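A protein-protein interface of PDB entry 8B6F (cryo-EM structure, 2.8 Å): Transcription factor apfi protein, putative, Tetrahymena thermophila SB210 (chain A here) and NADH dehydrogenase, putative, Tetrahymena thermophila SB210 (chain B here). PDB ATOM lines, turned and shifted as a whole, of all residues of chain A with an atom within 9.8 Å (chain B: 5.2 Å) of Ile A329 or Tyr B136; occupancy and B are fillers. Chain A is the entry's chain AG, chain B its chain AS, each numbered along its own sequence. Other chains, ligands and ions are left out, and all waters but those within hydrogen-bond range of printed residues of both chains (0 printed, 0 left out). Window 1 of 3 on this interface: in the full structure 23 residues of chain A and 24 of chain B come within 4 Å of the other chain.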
ATOM      1  N   ALA A 326      -9.066   1.615  -4.805  1.00  0.00           N
ATOM      2  CA  ALA A 326      -8.173   2.284  -5.744  1.00  0.00           C
ATOM      3  C   ALA A 326      -7.974   3.732  -5.314  1.00  0.00           C
ATOM      4  O   ALA A 326      -8.943   4.486  -5.187  1.00  0.00           O
ATOM      5  CB  ALA A 326      -8.741   2.213  -7.159  1.00  0.00           C
ATOM      6  N   THR A 327      -6.720   4.121  -5.100  1.00  0.00           N
ATOM      7  CA  THR A 327      -6.422   5.475  -4.657  1.00  0.00           C
ATOM      8  C   THR A 327      -6.720   6.478  -5.763  1.00  0.00           C
ATOM      9  O   THR A 327      -6.414   6.247  -6.936  1.00  0.00           O
ATOM     10  CB  THR A 327      -4.955   5.586  -4.238  1.00  0.00           C
ATOM     11  OG1 THR A 327      -4.664   4.609  -3.232  1.00  0.00           O
ATOM     12  CG2 THR A 327      -4.656   6.972  -3.685  1.00  0.00           C
ATOM     13  N   ILE A 328      -7.326   7.600  -5.383  1.00  0.00           N
ATOM     14  CA  ILE A 328      -7.627   8.693  -6.299  1.00  0.00           C
ATOM     15  C   ILE A 328      -6.942   9.946  -5.775  1.00  0.00           C
ATOM     16  O   ILE A 328      -7.146  10.331  -4.617  1.00  0.00           O
ATOM     17  CB  ILE A 328      -9.144   8.916  -6.442  1.00  0.00           C
ATOM     18  CG1 ILE A 328      -9.841   7.628  -6.892  1.00  0.00           C
ATOM     19  CG2 ILE A 328      -9.428  10.049  -7.420  1.00  0.00           C
ATOM     20  CD1 ILE A 328      -9.393   7.112  -8.246  1.00  0.00           C
ATOM     21  N   ILE A 329      -6.134  10.577  -6.622  1.00  0.00           N
ATOM     22  CA  ILE A 329      -5.424  11.802  -6.276  1.00  0.00           C
ATOM     23  C   ILE A 329      -6.251  12.977  -6.775  1.00  0.00           C
ATOM     24  O   ILE A 329      -6.572  13.059  -7.967  1.00  0.00           O
ATOM     25  CB  ILE A 329      -4.010  11.822  -6.877  1.00  0.00           C
ATOM     26  CG1 ILE A 329      -3.198  10.612  -6.399  1.00  0.00           C
ATOM     27  CG2 ILE A 329      -3.295  13.122  -6.527  1.00  0.00           C
ATOM     28  CD1 ILE A 329      -2.972  10.554  -4.902  1.00  0.00           C
ATOM     29  N   ASP A 330      -6.602  13.886  -5.867  1.00  0.00           N
ATOM     30  CA  ASP A 330      -7.423  15.031  -6.238  1.00  0.00           C
ATOM     31  C   ASP A 330      -6.710  15.887  -7.275  1.00  0.00           C
ATOM     32  O   ASP A 330      -5.525  16.200  -7.135  1.00  0.00           O
ATOM     33  CB  ASP A 330      -7.748  15.867  -5.000  1.00  0.00           C
ATOM     34  CG  ASP A 330      -8.546  15.094  -3.969  1.00  0.00           C
ATOM     35  OD1 ASP A 330      -8.807  13.893  -4.194  1.00  0.00           O
ATOM     36  OD2 ASP A 330      -8.912  15.686  -2.932  1.00  0.00           O
ATOM     37  N   ARG A 331      -7.441  16.263  -8.323  1.00  0.00           N
ATOM     38  CA  ARG A 331      -6.921  17.108  -9.388  1.00  0.00           C
ATOM     39  C   ARG A 331      -7.264  18.579  -9.197  1.00  0.00           C
ATOM     40  O   ARG A 331      -6.897  19.400 -10.043  1.00  0.00           O
ATOM     41  CB  ARG A 331      -7.459  16.634 -10.742  1.00  0.00           C
ATOM     42  CG  ARG A 331      -7.027  15.228 -11.130  1.00  0.00           C
ATOM     43  CD  ARG A 331      -5.638  15.216 -11.744  1.00  0.00           C
ATOM     44  NE  ARG A 331      -5.277  13.891 -12.235  1.00  0.00           N
ATOM     45  CZ  ARG A 331      -4.214  13.633 -12.984  1.00  0.00           C
ATOM     46  NH1 ARG A 331      -3.384  14.590 -13.361  1.00  0.00           N
ATOM     47  NH2 ARG A 331      -3.979  12.380 -13.366  1.00  0.00           N
ATOM     48  N   GLU A 332      -7.957  18.930  -8.117  1.00  0.00           N
ATOM     49  CA  GLU A 332      -8.347  20.316  -7.906  1.00  0.00           C
ATOM     50  C   GLU A 332      -7.114  21.197  -7.753  1.00  0.00           C
ATOM     51  O   GLU A 332      -6.149  20.832  -7.079  1.00  0.00           O
ATOM     52  CB  GLU A 332      -9.231  20.432  -6.663  1.00  0.00           C
ATOM     53  CG  GLU A 332     -10.523  19.631  -6.744  1.00  0.00           C
ATOM     54  CD  GLU A 332     -11.442  20.107  -7.852  1.00  0.00           C
ATOM     55  OE1 GLU A 332     -11.201  21.203  -8.401  1.00  0.00           O
ATOM     56  OE2 GLU A 332     -12.408  19.385  -8.177  1.00  0.00           O
ATOM     57  N   PHE A 333      -7.155  22.368  -8.384  1.00  0.00           N
ATOM     58  CA  PHE A 333      -6.026  23.286  -8.327  1.00  0.00           C
ATOM     59  C   PHE A 333      -5.717  23.659  -6.884  1.00  0.00           C
ATOM     60  O   PHE A 333      -6.614  24.002  -6.110  1.00  0.00           O
ATOM     61  CB  PHE A 333      -6.330  24.541  -9.142  1.00  0.00           C
ATOM     62  CG  PHE A 333      -5.342  25.654  -8.933  1.00  0.00           C
ATOM     63  CD1 PHE A 333      -4.180  25.714  -9.683  1.00  0.00           C
ATOM     64  CD2 PHE A 333      -5.582  26.645  -7.995  1.00  0.00           C
ATOM     65  CE1 PHE A 333      -3.271  26.738  -9.496  1.00  0.00           C
ATOM     66  CE2 PHE A 333      -4.677  27.671  -7.801  1.00  0.00           C
ATOM     67  CZ  PHE A 333      -3.520  27.718  -8.553  1.00  0.00           C
ATOM     68  N   LYS A 334      -4.438  23.593  -6.528  1.00  0.00           N
ATOM     69  CA  LYS A 334      -3.970  23.958  -5.201  1.00  0.00           C
ATOM     70  C   LYS A 334      -2.746  24.850  -5.337  1.00  0.00           C
ATOM     71  O   LYS A 334      -1.911  24.639  -6.220  1.00  0.00           O
ATOM     72  CB  LYS A 334      -3.629  22.715  -4.369  1.00  0.00           C
ATOM     73  CG  LYS A 334      -3.140  23.026  -2.964  1.00  0.00           C
ATOM     74  CD  LYS A 334      -2.814  21.754  -2.197  1.00  0.00           C
ATOM     75  CE  LYS A 334      -2.295  22.071  -0.802  1.00  0.00           C
ATOM     76  NZ  LYS A 334      -1.934  20.839  -0.045  1.00  0.00           N
ATOM     77  N   ASN B  88       5.822  12.930  -8.335  1.00  0.00           N
ATOM     78  CA  ASN B  88       4.720  12.824  -9.286  1.00  0.00           C
ATOM     79  C   ASN B  88       4.598  11.408  -9.833  1.00  0.00           C
ATOM     80  O   ASN B  88       3.490  10.871  -9.938  1.00  0.00           O
ATOM     81  CB  ASN B  88       4.913  13.826 -10.423  1.00  0.00           C
ATOM     82  CG  ASN B  88       4.934  15.258  -9.933  1.00  0.00           C
ATOM     83  OD1 ASN B  88       4.308  15.590  -8.930  1.00  0.00           O
ATOM     84  ND2 ASN B  88       5.654  16.115 -10.644  1.00  0.00           N
ATOM     85  N   ASN B  91       3.042   9.298  -7.233  1.00  0.00           N
ATOM     86  CA  ASN B  91       1.588   9.408  -7.257  1.00  0.00           C
ATOM     87  C   ASN B  91       1.001   8.574  -8.386  1.00  0.00           C
ATOM     88  O   ASN B  91      -0.042   7.933  -8.217  1.00  0.00           O
ATOM     89  CB  ASN B  91       1.166  10.870  -7.405  1.00  0.00           C
ATOM     90  CG  ASN B  91       1.421  11.678  -6.153  1.00  0.00           C
ATOM     91  OD1 ASN B  91       1.411  11.146  -5.045  1.00  0.00           O
ATOM     92  ND2 ASN B  91       1.646  12.975  -6.323  1.00  0.00           N
ATOM     93  N   TYR B  92       1.651   8.579  -9.549  1.00  0.00           N
ATOM     94  CA  TYR B  92       1.201   7.733 -10.646  1.00  0.00           C
ATOM     95  C   TYR B  92       1.155   6.270 -10.219  1.00  0.00           C
ATOM     96  O   TYR B  92       0.184   5.562 -10.506  1.00  0.00           O
ATOM     97  CB  TYR B  92       2.123   7.919 -11.852  1.00  0.00           C
ATOM     98  CG  TYR B  92       1.718   7.122 -13.067  1.00  0.00           C
ATOM     99  CD1 TYR B  92       2.156   5.819 -13.249  1.00  0.00           C
ATOM    100  CD2 TYR B  92       0.902   7.681 -14.039  1.00  0.00           C
ATOM    101  CE1 TYR B  92       1.787   5.091 -14.361  1.00  0.00           C
ATOM    102  CE2 TYR B  92       0.527   6.964 -15.154  1.00  0.00           C
ATOM    103  CZ  TYR B  92       0.972   5.670 -15.311  1.00  0.00           C
ATOM    104  OH  TYR B  92       0.599   4.953 -16.422  1.00  0.00           O
ATOM    105  N   GLU B  95      -1.736   5.551  -7.663  1.00  0.00           N
ATOM    106  CA  GLU B  95      -3.036   5.355  -8.293  1.00  0.00           C
ATOM    107  C   GLU B  95      -3.217   3.917  -8.764  1.00  0.00           C
ATOM    108  O   GLU B  95      -4.348   3.424  -8.825  1.00  0.00           O
ATOM    109  CB  GLU B  95      -3.199   6.323  -9.460  1.00  0.00           C
ATOM    110  CG  GLU B  95      -3.430   7.752  -9.022  1.00  0.00           C
ATOM    111  CD  GLU B  95      -3.660   8.680 -10.189  1.00  0.00           C
ATOM    112  OE1 GLU B  95      -3.055   8.451 -11.258  1.00  0.00           O
ATOM    113  OE2 GLU B  95      -4.451   9.635 -10.043  1.00  0.00           O
ATOM    114  N   ARG B  96      -2.124   3.234  -9.102  1.00  0.00           N
ATOM    115  CA  ARG B  96      -2.169   1.850  -9.556  1.00  0.00           C
ATOM    116  C   ARG B  96      -1.821   0.848  -8.462  1.00  0.00           C
ATOM    117  O   ARG B  96      -1.762  -0.353  -8.743  1.00  0.00           O
ATOM    118  CB  ARG B  96      -1.214   1.652 -10.741  1.00  0.00           C
ATOM    119  CG  ARG B  96      -1.751   2.135 -12.082  1.00  0.00           C
ATOM    120  CD  ARG B  96      -1.752   3.651 -12.185  1.00  0.00           C
ATOM    121  NE  ARG B  96      -2.194   4.110 -13.496  1.00  0.00           N
ATOM    122  CZ  ARG B  96      -2.338   5.383 -13.835  1.00  0.00           C
ATOM    123  NH1 ARG B  96      -2.084   6.360 -12.979  1.00  0.00           N
ATOM    124  NH2 ARG B  96      -2.754   5.687 -15.062  1.00  0.00           N
ATOM    125  N   SER B 134       4.290  15.313 -14.644  1.00  0.00           N
ATOM    126  CA  SER B 134       3.631  16.564 -14.313  1.00  0.00           C
ATOM    127  C   SER B 134       2.914  16.461 -12.966  1.00  0.00           C
ATOM    128  O   SER B 134       2.406  15.397 -12.605  1.00  0.00           O
ATOM    129  CB  SER B 134       2.626  16.940 -15.397  1.00  0.00           C
ATOM    130  OG  SER B 134       3.260  17.072 -16.657  1.00  0.00           O
ATOM    131  N   PRO B 135       2.852  17.556 -12.205  1.00  0.00           N
ATOM    132  CA  PRO B 135       2.123  17.518 -10.933  1.00  0.00           C
ATOM    133  C   PRO B 135       0.636  17.275 -11.146  1.00  0.00           C
ATOM    134  O   PRO B 135       0.052  17.691 -12.147  1.00  0.00           O
ATOM    135  CB  PRO B 135       2.378  18.904 -10.329  1.00  0.00           C
ATOM    136  CG  PRO B 135       3.561  19.435 -11.049  1.00  0.00           C
ATOM    137  CD  PRO B 135       3.495  18.863 -12.422  1.00  0.00           C
ATOM    138  N   TYR B 136       0.022  16.594 -10.177  1.00  0.00           N
ATOM    139  CA  TYR B 136      -1.402  16.290 -10.270  1.00  0.00           C
ATOM    140  C   TYR B 136      -2.266  17.505  -9.958  1.00  0.00           C
ATOM    141  O   TYR B 136      -3.299  17.714 -10.603  1.00  0.00           O
ATOM    142  CB  TYR B 136      -1.752  15.136  -9.331  1.00  0.00           C
ATOM    143  CG  TYR B 136      -1.486  13.777  -9.930  1.00  0.00           C
ATOM    144  CD1 TYR B 136      -0.192  13.355 -10.203  1.00  0.00           C
ATOM    145  CD2 TYR B 136      -2.531  12.914 -10.223  1.00  0.00           C
ATOM    146  CE1 TYR B 136       0.051  12.114 -10.753  1.00  0.00           C
ATOM    147  CE2 TYR B 136      -2.299  11.672 -10.772  1.00  0.00           C
ATOM    148  CZ  TYR B 136      -1.007  11.276 -11.033  1.00  0.00           C
ATOM    149  OH  TYR B 136      -0.775  10.038 -11.581  1.00  0.00           O
ATOM    150  N   ASN B 137      -1.865  18.316  -8.977  1.00  0.00           N
ATOM    151  CA  ASN B 137      -2.667  19.464  -8.574  1.00  0.00           C
ATOM    152  C   ASN B 137      -1.832  20.715  -8.332  1.00  0.00           C
ATOM    153  O   ASN B 137      -2.370  21.707  -7.826  1.00  0.00           O
ATOM    154  CB  ASN B 137      -3.470  19.133  -7.312  1.00  0.00           C
ATOM    155  CG  ASN B 137      -2.594  18.676  -6.167  1.00  0.00           C
ATOM    156  OD1 ASN B 137      -1.548  18.064  -6.378  1.00  0.00           O
ATOM    157  ND2 ASN B 137      -3.019  18.968  -4.944  1.00  0.00           N
ATOM    158  N   THR B 138      -0.549  20.708  -8.682  1.00  0.00           N
ATOM    159  CA  THR B 138       0.326  21.846  -8.468  1.00  0.00           C
ATOM    160  C   THR B 138       0.700  22.487  -9.803  1.00  0.00           C
ATOM    161  O   THR B 138       0.826  21.790 -10.814  1.00  0.00           O
ATOM    162  CB  THR B 138       1.605  21.415  -7.737  1.00  0.00           C
ATOM    163  OG1 THR B 138       1.260  20.731  -6.525  1.00  0.00           O
ATOM    164  CG2 THR B 138       2.480  22.616  -7.406  1.00  0.00           C
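The backbone NH of Lys A334 is in hydrogen-bond range of the backbone carbonyl oxygen of Asn B137 (3.1 Å).
The side-chain hydroxyl (OH) of Tyr B136 sits close to the backbone NH (N) of Tyr B92 (3.5 Å). The guanidinium group (NH1) of Arg B96 lies within salt-bridge range of the side-chain carboxylate (OE1) of Glu B95 (2.9 Å). The side-chain carboxylate (OE1) of Glu B95 sits at hydrogen-bond distance from the side-chain hydroxyl (OH) of Tyr B136, at 2.8 Å.
Among the printed residues, pairs that only touch across the chains: Arg A331 with Tyr B136 (3.2 Å), Glu A332 with Asn B137 (3.2 Å), Asp A330 with Asn B137 (3.6 Å), Thr A327 with Glu B95 (3.7 Å), Ile A329 with Tyr B136 (3.8 Å), Ile A329 with Glu B95 (3.9 Å) and Phe A333 with Asn B137 (3.99 Å).
Of chain A, only Ile A329 and Arg A331 come within 4 Å of Tyr B136. No residue of chain A comes within 4 Å of Asn B91. No residue of chain A comes within 4 Å of Pro B135. Of the printed residues of chain B, Arg A331 touches Tyr B136. Of the printed residues of chain B, Phe A333 touches Asn B137. Of the printed residues of chain A, Asn B137 touches Asp A330 (3.6 Å), Glu A332 (3.2 Å), Phe A333 (3.99 Å) and Lys A334 (3.1 Å). Of the printed residues of chain B, Thr A327 touches Glu B95 (3.7 Å). Of the printed residues of chain B, Asp A330 touches Asn B137 (3.6 Å). Ile A328 touches none of the printed residues of chain B. The nearest printed residue of chain B that does not touch Arg A331 is Asn B137 (4.3 Å).
Of the 9 printed residues of chain A, 7 touch a printed residue of chain B. Hydrophobic or aromatic side chains of chain A that line the printed part of chain B: Ile A329. Of the 10 printed residues of chain B, 3 touch a printed residue of chain A. Along chain B the printed residues that touch a printed residue of chain A span positions 95 to 137. Among the printed residues, 8 pairs touch across the chains.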
